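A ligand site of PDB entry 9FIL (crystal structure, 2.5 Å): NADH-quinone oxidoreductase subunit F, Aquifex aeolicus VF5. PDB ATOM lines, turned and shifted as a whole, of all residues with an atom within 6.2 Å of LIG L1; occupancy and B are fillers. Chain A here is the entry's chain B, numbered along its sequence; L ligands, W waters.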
ATOM      1  N   GLY A  67       4.551  21.309   7.504  1.00  0.00           N
ATOM      2  CA  GLY A  67       3.212  20.955   7.053  1.00  0.00           C
ATOM      3  C   GLY A  67       3.140  20.872   5.533  1.00  0.00           C
ATOM      4  O   GLY A  67       2.087  20.529   4.990  1.00  0.00           O
ATOM      5  N   GLY A  68       4.247  21.265   4.876  1.00  0.00           N
ATOM      6  CA  GLY A  68       4.530  20.879   3.503  1.00  0.00           C
ATOM      7  C   GLY A  68       4.719  22.040   2.522  1.00  0.00           C
ATOM      8  O   GLY A  68       4.963  21.782   1.335  1.00  0.00           O
ATOM      9  N   ALA A  69       4.598  23.304   2.981  1.00  0.00           N
ATOM     10  CA  ALA A  69       4.831  24.438   2.094  1.00  0.00           C
ATOM     11  C   ALA A  69       6.211  25.066   2.324  1.00  0.00           C
ATOM     12  O   ALA A  69       6.686  25.822   1.501  1.00  0.00           O
ATOM     13  CB  ALA A  69       3.717  25.443   2.255  1.00  0.00           C
ATOM     14  N   GLY A  70       6.842  24.751   3.471  1.00  0.00           N
ATOM     15  CA  GLY A  70       8.245  25.106   3.706  1.00  0.00           C
ATOM     16  C   GLY A  70       8.466  26.596   3.932  1.00  0.00           C
ATOM     17  O   GLY A  70       9.546  27.105   3.638  1.00  0.00           O
ATOM     18  N   PHE A  71       7.468  27.306   4.488  1.00  0.00           N
ATOM     19  CA  PHE A  71       7.612  28.722   4.773  1.00  0.00           C
ATOM     20  C   PHE A  71       8.504  28.949   5.998  1.00  0.00           C
ATOM     21  O   PHE A  71       8.286  28.328   7.039  1.00  0.00           O
ATOM     22  CB  PHE A  71       6.275  29.401   5.034  1.00  0.00           C
ATOM     23  CG  PHE A  71       6.346  30.916   4.929  1.00  0.00           C
ATOM     24  CD1 PHE A  71       6.219  31.541   3.690  1.00  0.00           C
ATOM     25  CD2 PHE A  71       6.542  31.713   6.056  1.00  0.00           C
ATOM     26  CE1 PHE A  71       6.290  32.923   3.586  1.00  0.00           C
ATOM     27  CE2 PHE A  71       6.585  33.093   5.950  1.00  0.00           C
ATOM     28  CZ  PHE A  71       6.467  33.698   4.707  1.00  0.00           C
ATOM     29  N   LYS A  76       7.705  33.985   9.661  1.00  0.00           N
ATOM     30  CA  LYS A  76       6.278  33.923   9.924  1.00  0.00           C
ATOM     31  C   LYS A  76       5.960  34.587  11.262  1.00  0.00           C
ATOM     32  O   LYS A  76       4.996  35.339  11.353  1.00  0.00           O
ATOM     33  CB  LYS A  76       5.734  32.493   9.877  1.00  0.00           C
ATOM     34  CG  LYS A  76       4.224  32.429  10.044  1.00  0.00           C
ATOM     35  CD  LYS A  76       3.636  31.052  10.303  1.00  0.00           C
ATOM     36  CE  LYS A  76       3.594  30.278   9.045  1.00  0.00           C
ATOM     37  NZ  LYS A  76       3.211  28.871   9.217  1.00  0.00           N
ATOM     38  N   PHE A  79       6.205  38.414  11.152  1.00  0.00           N
ATOM     39  CA  PHE A  79       5.065  39.052  10.534  1.00  0.00           C
ATOM     40  C   PHE A  79       3.940  39.220  11.548  1.00  0.00           C
ATOM     41  O   PHE A  79       3.320  40.284  11.635  1.00  0.00           O
ATOM     42  CB  PHE A  79       4.639  38.232   9.303  1.00  0.00           C
ATOM     43  CG  PHE A  79       5.469  38.378   8.026  1.00  0.00           C
ATOM     44  CD1 PHE A  79       6.167  39.551   7.743  1.00  0.00           C
ATOM     45  CD2 PHE A  79       5.501  37.358   7.092  1.00  0.00           C
ATOM     46  CE1 PHE A  79       6.884  39.672   6.555  1.00  0.00           C
ATOM     47  CE2 PHE A  79       6.224  37.483   5.915  1.00  0.00           C
ATOM     48  CZ  PHE A  79       6.916  38.636   5.645  1.00  0.00           C
ATOM     49  N   GLU A  97      -3.491  13.529   5.357  1.00  0.00           N
ATOM     50  CA  GLU A  97      -3.061  13.210   4.012  1.00  0.00           C
ATOM     51  C   GLU A  97      -2.665  11.735   3.971  1.00  0.00           C
ATOM     52  O   GLU A  97      -1.965  11.225   4.856  1.00  0.00           O
ATOM     53  CB  GLU A  97      -1.883  14.069   3.563  1.00  0.00           C
ATOM     54  CG  GLU A  97      -1.801  14.266   2.055  1.00  0.00           C
ATOM     55  CD  GLU A  97      -0.465  14.791   1.537  1.00  0.00           C
ATOM     56  OE1 GLU A  97       0.177  15.611   2.232  1.00  0.00           O
ATOM     57  OE2 GLU A  97      -0.102  14.380   0.399  1.00  0.00           O
ATOM     58  N   TYR A 180     -10.261  16.478   5.826  1.00  0.00           N
ATOM     59  CA  TYR A 180      -8.865  16.770   5.548  1.00  0.00           C
ATOM     60  C   TYR A 180      -8.660  18.270   5.329  1.00  0.00           C
ATOM     61  O   TYR A 180      -7.557  18.774   5.549  1.00  0.00           O
ATOM     62  CB  TYR A 180      -8.480  15.884   4.357  1.00  0.00           C
ATOM     63  CG  TYR A 180      -7.232  16.268   3.582  1.00  0.00           C
ATOM     64  CD1 TYR A 180      -5.965  15.966   4.055  1.00  0.00           C
ATOM     65  CD2 TYR A 180      -7.331  16.896   2.345  1.00  0.00           C
ATOM     66  CE1 TYR A 180      -4.832  16.308   3.333  1.00  0.00           C
ATOM     67  CE2 TYR A 180      -6.218  17.231   1.611  1.00  0.00           C
ATOM     68  CZ  TYR A 180      -4.955  16.947   2.111  1.00  0.00           C
ATOM     69  OH  TYR A 180      -3.822  17.259   1.420  1.00  0.00           O
ATOM     70  N   GLU A 184      -5.886  22.479   6.262  1.00  0.00           N
ATOM     71  CA  GLU A 184      -5.555  23.765   5.656  1.00  0.00           C
ATOM     72  C   GLU A 184      -5.756  24.816   6.746  1.00  0.00           C
ATOM     73  O   GLU A 184      -6.746  24.735   7.468  1.00  0.00           O
ATOM     74  CB  GLU A 184      -6.358  23.947   4.372  1.00  0.00           C
ATOM     75  CG  GLU A 184      -5.861  25.111   3.528  1.00  0.00           C
ATOM     76  CD  GLU A 184      -6.375  26.479   3.940  1.00  0.00           C
ATOM     77  OE1 GLU A 184      -7.370  26.494   4.679  1.00  0.00           O
ATOM     78  OE2 GLU A 184      -5.805  27.515   3.518  1.00  0.00           O
ATOM     79  N   GLU A 185      -4.792  25.728   6.900  1.00  0.00           N
ATOM     80  CA  GLU A 185      -4.681  26.572   8.103  1.00  0.00           C
ATOM     81  C   GLU A 185      -5.916  27.461   8.322  1.00  0.00           C
ATOM     82  O   GLU A 185      -6.355  27.588   9.456  1.00  0.00           O
ATOM     83  CB  GLU A 185      -3.382  27.373   8.089  1.00  0.00           C
ATOM     84  CG  GLU A 185      -3.312  28.383   6.954  1.00  0.00           C
ATOM     85  CD  GLU A 185      -2.087  29.278   6.862  1.00  0.00           C
ATOM     86  OE1 GLU A 185      -1.285  29.388   7.828  1.00  0.00           O
ATOM     87  OE2 GLU A 185      -1.957  29.899   5.778  1.00  0.00           O
ATOM     88  N   LYS A 202      -6.990  33.932   0.898  1.00  0.00           N
ATOM     89  CA  LYS A 202      -5.732  34.485   1.369  1.00  0.00           C
ATOM     90  C   LYS A 202      -5.055  35.203   0.202  1.00  0.00           C
ATOM     91  O   LYS A 202      -5.210  34.766  -0.941  1.00  0.00           O
ATOM     92  CB  LYS A 202      -4.783  33.388   1.830  1.00  0.00           C
ATOM     93  CG  LYS A 202      -5.267  32.538   2.995  1.00  0.00           C
ATOM     94  CD  LYS A 202      -4.661  31.140   2.983  1.00  0.00           C
ATOM     95  CE  LYS A 202      -3.156  31.077   2.944  1.00  0.00           C
ATOM     96  NZ  LYS A 202      -2.673  29.687   2.943  1.00  0.00           N
ATOM     97  N   TYR A 205      -3.228  36.622   5.312  1.00  0.00           N
ATOM     98  CA  TYR A 205      -2.639  35.446   5.955  1.00  0.00           C
ATOM     99  C   TYR A 205      -3.076  35.468   7.414  1.00  0.00           C
ATOM    100  O   TYR A 205      -3.414  36.519   7.926  1.00  0.00           O
ATOM    101  CB  TYR A 205      -1.111  35.425   5.777  1.00  0.00           C
ATOM    102  CG  TYR A 205      -0.733  35.144   4.337  1.00  0.00           C
ATOM    103  CD1 TYR A 205      -0.919  33.883   3.789  1.00  0.00           C
ATOM    104  CD2 TYR A 205      -0.229  36.151   3.520  1.00  0.00           C
ATOM    105  CE1 TYR A 205      -0.618  33.630   2.456  1.00  0.00           C
ATOM    106  CE2 TYR A 205       0.070  35.905   2.193  1.00  0.00           C
ATOM    107  CZ  TYR A 205      -0.131  34.644   1.660  1.00  0.00           C
ATOM    108  OH  TYR A 205       0.172  34.413   0.350  1.00  0.00           O
ATOM    109  N   PRO A 206      -3.077  34.322   8.134  1.00  0.00           N
ATOM    110  CA  PRO A 206      -3.504  34.316   9.526  1.00  0.00           C
ATOM    111  C   PRO A 206      -2.693  35.203  10.468  1.00  0.00           C
ATOM    112  O   PRO A 206      -3.227  35.657  11.469  1.00  0.00           O
ATOM    113  CB  PRO A 206      -3.423  32.806   9.896  1.00  0.00           C
ATOM    114  CG  PRO A 206      -3.466  32.094   8.576  1.00  0.00           C
ATOM    115  CD  PRO A 206      -2.642  32.996   7.670  1.00  0.00           C
ATOM    116  N   VAL A 207      -1.411  35.451  10.150  1.00  0.00           N
ATOM    117  CA  VAL A 207      -0.515  36.261  10.972  1.00  0.00           C
ATOM    118  C   VAL A 207      -1.017  37.706  11.032  1.00  0.00           C
ATOM    119  O   VAL A 207      -0.659  38.453  11.941  1.00  0.00           O
ATOM    120  CB  VAL A 207       0.950  36.219  10.503  1.00  0.00           C
ATOM    121  CG1 VAL A 207       1.590  34.863  10.760  1.00  0.00           C
ATOM    122  CG2 VAL A 207       1.107  36.607   9.033  1.00  0.00           C
ATOM    123  N   VAL A 218      -0.124  29.677  12.682  1.00  0.00           N
ATOM    124  CA  VAL A 218      -0.385  28.260  12.576  1.00  0.00           C
ATOM    125  C   VAL A 218       0.921  27.585  12.184  1.00  0.00           C
ATOM    126  O   VAL A 218       1.537  27.992  11.196  1.00  0.00           O
ATOM    127  CB  VAL A 218      -1.510  27.952  11.552  1.00  0.00           C
ATOM    128  CG1 VAL A 218      -1.747  26.448  11.442  1.00  0.00           C
ATOM    129  CG2 VAL A 218      -2.798  28.681  11.920  1.00  0.00           C
ATOM    130  N   LEU A 297      -0.044  13.915  -3.638  1.00  0.00           N
ATOM    131  CA  LEU A 297       0.482  15.099  -4.294  1.00  0.00           C
ATOM    132  C   LEU A 297       1.183  14.784  -5.629  1.00  0.00           C
ATOM    133  O   LEU A 297       0.952  15.472  -6.614  1.00  0.00           O
ATOM    134  CB  LEU A 297       1.465  15.755  -3.316  1.00  0.00           C
ATOM    135  CG  LEU A 297       2.030  17.133  -3.717  1.00  0.00           C
ATOM    136  CD1 LEU A 297       0.945  18.202  -3.690  1.00  0.00           C
ATOM    137  CD2 LEU A 297       3.202  17.573  -2.818  1.00  0.00           C
ATOM    138  N   GLY A 318       7.375  18.022  -1.179  1.00  0.00           N
ATOM    139  CA  GLY A 318       6.177  17.616  -0.449  1.00  0.00           C
ATOM    140  C   GLY A 318       6.457  17.513   1.044  1.00  0.00           C
ATOM    141  O   GLY A 318       6.989  18.443   1.647  1.00  0.00           O
ATOM    142  N   THR A 319       6.107  16.359   1.624  1.00  0.00           N
ATOM    143  CA  THR A 319       6.339  16.114   3.045  1.00  0.00           C
ATOM    144  C   THR A 319       7.223  14.882   3.227  1.00  0.00           C
ATOM    145  O   THR A 319       7.294  14.365   4.332  1.00  0.00           O
ATOM    146  CB  THR A 319       4.981  15.949   3.745  1.00  0.00           C
ATOM    147  OG1 THR A 319       4.198  14.997   3.030  1.00  0.00           O
ATOM    148  CG2 THR A 319       4.177  17.233   3.789  1.00  0.00           C
ATOM    149  N   CYS A 393      -8.046  27.434  -2.162  1.00  0.00           N
ATOM    150  CA  CYS A 393      -7.006  26.733  -1.394  1.00  0.00           C
ATOM    151  C   CYS A 393      -6.280  25.738  -2.293  1.00  0.00           C
ATOM    152  O   CYS A 393      -6.575  25.641  -3.487  1.00  0.00           O
ATOM    153  CB  CYS A 393      -7.508  26.070  -0.113  1.00  0.00           C
ATOM    154  SG  CYS A 393      -8.167  24.396  -0.316  1.00  0.00           S
ATOM    155  N   GLY A 394      -5.310  25.028  -1.683  1.00  0.00           N
ATOM    156  CA  GLY A 394      -4.335  24.203  -2.386  1.00  0.00           C
ATOM    157  C   GLY A 394      -4.859  22.830  -2.789  1.00  0.00           C
ATOM    158  O   GLY A 394      -4.281  22.195  -3.676  1.00  0.00           O
ATOM    159  N   VAL A 398      -4.174  20.923  -6.415  1.00  0.00           N
ATOM    160  CA  VAL A 398      -3.413  19.687  -6.588  1.00  0.00           C
ATOM    161  C   VAL A 398      -4.283  18.461  -6.901  1.00  0.00           C
ATOM    162  O   VAL A 398      -3.750  17.387  -7.188  1.00  0.00           O
ATOM    163  CB  VAL A 398      -2.547  19.416  -5.333  1.00  0.00           C
ATOM    164  CG1 VAL A 398      -1.640  20.596  -4.972  1.00  0.00           C
ATOM    165  CG2 VAL A 398      -3.390  19.004  -4.130  1.00  0.00           C
HETATM  166  P1  LIG L   1       1.176  28.509   1.376  1.00  0.00           P
HETATM  167  O1  LIG L   1       2.437  28.647   0.598  1.00  0.00           O
HETATM  168  O2  LIG L   1       0.011  29.315   0.904  1.00  0.00           O
HETATM  169  O3  LIG L   1       1.470  28.919   2.890  1.00  0.00           O
HETATM  170  C1  LIG L   1       2.347  28.136   3.727  1.00  0.00           C
HETATM  171  C2  LIG L   1       2.437  28.766   5.097  1.00  0.00           C
HETATM  172  O4  LIG L   1       3.189  30.002   4.996  1.00  0.00           O
HETATM  173  C3  LIG L   1       1.106  29.192   5.732  1.00  0.00           C
HETATM  174  O5  LIG L   1       1.181  29.210   7.146  1.00  0.00           O
HETATM  175  C4  LIG L   1       0.950  30.609   5.202  1.00  0.00           C
HETATM  176  O6  LIG L   1       0.072  31.453   5.920  1.00  0.00           O
HETATM  177  C5  LIG L   1       2.377  31.108   5.328  1.00  0.00           C
HETATM  178  N1  LIG L   1       2.661  32.234   4.429  1.00  0.00           N
HETATM  179  C6  LIG L   1       2.922  32.160   3.083  1.00  0.00           C
HETATM  180  N2  LIG L   1       3.117  33.329   2.533  1.00  0.00           N
HETATM  181  C7  LIG L   1       2.987  34.224   3.586  1.00  0.00           C
HETATM  182  C8  LIG L   1       3.107  35.618   3.632  1.00  0.00           C
HETATM  183  N3  LIG L   1       3.391  36.364   2.580  1.00  0.00           N
HETATM  184  N4  LIG L   1       2.911  36.211   4.829  1.00  0.00           N
HETATM  185  C9  LIG L   1       2.622  35.436   5.888  1.00  0.00           C
HETATM  186  N5  LIG L   1       2.489  34.119   5.965  1.00  0.00           N
HETATM  187  C10 LIG L   1       2.683  33.558   4.754  1.00  0.00           C
HETATM  188  O7  LIG L   1       0.733  26.975   1.508  1.00  0.00           O
HETATM  189  P2  LIG L   1      -0.545  26.248   2.177  1.00  0.00           P
HETATM  190  O8  LIG L   1      -1.777  26.430   1.331  1.00  0.00           O
HETATM  191  O9  LIG L   1      -0.631  26.670   3.604  1.00  0.00           O
HETATM  192  O10 LIG L   1      -0.123  24.683   2.115  1.00  0.00           O
HETATM  193  C11 LIG L   1      -0.153  23.919   0.864  1.00  0.00           C
HETATM  194  C12 LIG L   1       0.656  22.642   0.983  1.00  0.00           C
HETATM  195  O11 LIG L   1       0.544  22.093   2.321  1.00  0.00           O
HETATM  196  C13 LIG L   1       0.208  21.463   0.094  1.00  0.00           C
HETATM  197  O12 LIG L   1       0.639  21.600  -1.258  1.00  0.00           O
HETATM  198  C14 LIG L   1       0.845  20.252   0.808  1.00  0.00           C
HETATM  199  O13 LIG L   1       2.226  20.032   0.527  1.00  0.00           O
HETATM  200  C15 LIG L   1       0.649  20.662   2.282  1.00  0.00           C
HETATM  201  N6  LIG L   1      -0.564  20.083   2.921  1.00  0.00           N
HETATM  202  C1  LG2 L   2      -2.558  21.678   4.633  1.00  0.00           C
HETATM  203  N1  LG2 L   2      -1.546  21.951   5.606  1.00  0.00           N
HETATM  204  C2  LG2 L   2      -1.394  21.065   6.659  1.00  0.00           C
HETATM  205  N2  LG2 L   2      -0.470  21.354   7.639  1.00  0.00           N
HETATM  206  C3  LG2 L   2      -0.357  20.618   8.784  1.00  0.00           C
HETATM  207  O1  LG2 L   2       0.337  20.961   9.709  1.00  0.00           O
HETATM  208  N3  LG2 L   2      -1.127  19.506   8.853  1.00  0.00           N
HETATM  209  C4  LG2 L   2      -2.040  19.082   7.922  1.00  0.00           C
HETATM  210  O2  LG2 L   2      -2.652  18.048   8.119  1.00  0.00           O
HETATM  211  C5  LG2 L   2      -2.161  19.937   6.793  1.00  0.00           C
HETATM  212  N4  LG2 L   2      -3.089  19.659   5.852  1.00  0.00           N
HETATM  213  C6  LG2 L   2      -3.323  20.518   4.781  1.00  0.00           C
HETATM  214  C7  LG2 L   2      -4.322  20.225   3.845  1.00  0.00           C
HETATM  215  C8  LG2 L   2      -4.546  21.065   2.770  1.00  0.00           C
HETATM  216  C9  LG2 L   2      -5.565  20.655   1.728  1.00  0.00           C
HETATM  217  C10 LG2 L   2      -3.788  22.228   2.616  1.00  0.00           C
HETATM  218  C11 LG2 L   2      -4.000  23.161   1.450  1.00  0.00           C
HETATM  219  C12 LG2 L   2      -2.791  22.529   3.557  1.00  0.00           C
HETATM  220  C13 LG2 L   2      -0.702  23.146   5.482  1.00  0.00           C
HETATM  221  C14 LG2 L   2      -1.333  24.344   6.194  1.00  0.00           C
HETATM  222  O3  LG2 L   2      -2.119  25.093   5.264  1.00  0.00           O
HETATM  223  C15 LG2 L   2      -0.222  25.234   6.772  1.00  0.00           C
HETATM  224  O4  LG2 L   2       0.865  25.371   5.871  1.00  0.00           O
HETATM  225  C16 LG2 L   2       0.334  24.722   8.101  1.00  0.00           C
HETATM  226  O5  LG2 L   2      -0.720  24.579   9.041  1.00  0.00           O
HETATM  227  C17 LG2 L   2       1.400  25.639   8.661  1.00  0.00           C
HETATM  228  O6  LG2 L   2       2.498  24.744   8.759  1.00  0.00           O
HETATM  229  P1  LG2 L   2       4.048  25.134   8.980  1.00  0.00           P
HETATM  230  O7  LG2 L   2       4.184  24.933  10.458  1.00  0.00           O
HETATM  231  O8  LG2 L   2       4.392  26.524   8.497  1.00  0.00           O
HETATM  232  O9  LG2 L   2       4.706  24.062   8.147  1.00  0.00           O
HETATM  233  O   HOH W   1      -1.647  17.568   2.733  1.00  0.00           O
HETATM  234  O   HOH W   2       0.760  32.839   8.077  1.00  0.00           O
HETATM  235  O   HOH W   3       4.891  26.563   5.669  1.00  0.00           O
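The side-chain carboxylate of Glu 185 is in salt-bridge range of the side-chain amino group of Lys 202 (2.9 Å).
NZ of Lys 76 lies within hydrogen-bond range of O of Val 218 (2.7 Å).
OE2 of Glu 184 is in salt-bridge range of NZ of Lys 202, 3.9 Å away.
O of Gly 67 sits close to N6 of LIG L1 (3.4 Å).
Residues that only touch LIG L1: Phe 71, Ala 69, Tyr 205, Pro 206, Phe 79 and Val 207.
Hydrophobic or aromatic side chains within 4 Å of LIG L1: Ala 69, Phe 71, Phe 79, Tyr 205, Pro 206 and Val 207.
Within 4 Å of LIG L1: Gly 67, Gly 68, Ala 69, Phe 71, Lys 76, Phe 79, Glu 185, Lys 202, Tyr 205, Pro 206 and Val 207.
The side-chain carboxylate (OE2) of Glu 185 is in hydrogen-bond range of an oxygen (O6) of LIG L1.
An oxygen (O5) of LIG L1 sits at hydrogen-bond distance from the side-chain amino group of Lys 76 (2.9 Å).
An oxygen (O13) of LIG L1 is in hydrogen-bond range of the backbone carbonyl oxygen (O) of Gly 68, 3.3 Å away.
An oxygen (O2) of LIG L1 is in salt-bridge range of the side-chain amino group (NZ) of Lys 202, at 3.4 Å.
The backbone NH (N) of Glu 185 lies within hydrogen-bond range of an oxygen (O3) of LG2 L2 (3.2 Å).
The side-chain amino group of Lys 76 lies within salt-bridge range of an oxygen (O8) of LG2 L2 (2.7 Å).
An oxygen (O9) of LG2 L2 lies within hydrogen-bond range of the backbone NH (N) of Gly 67 (2.8 Å).
An oxygen (O9) of LIG L1 is in hydrogen-bond range of an oxygen (O3) of LG2 L2, 2.7 Å away.
Water W1 lies within hydrogen-bond range of the side-chain hydroxyl of Tyr 180 (2.6 Å), the side-chain carboxylate of Glu 97 (2.7 Å) and a nitrogen (N6) of LIG L1 (2.7 Å).
Water W3 lies within hydrogen-bond range of O8 of LG2 L2 (2.9 Å), N of Phe 71 (2.9 Å) and N of Gly 70 (3.5 Å).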
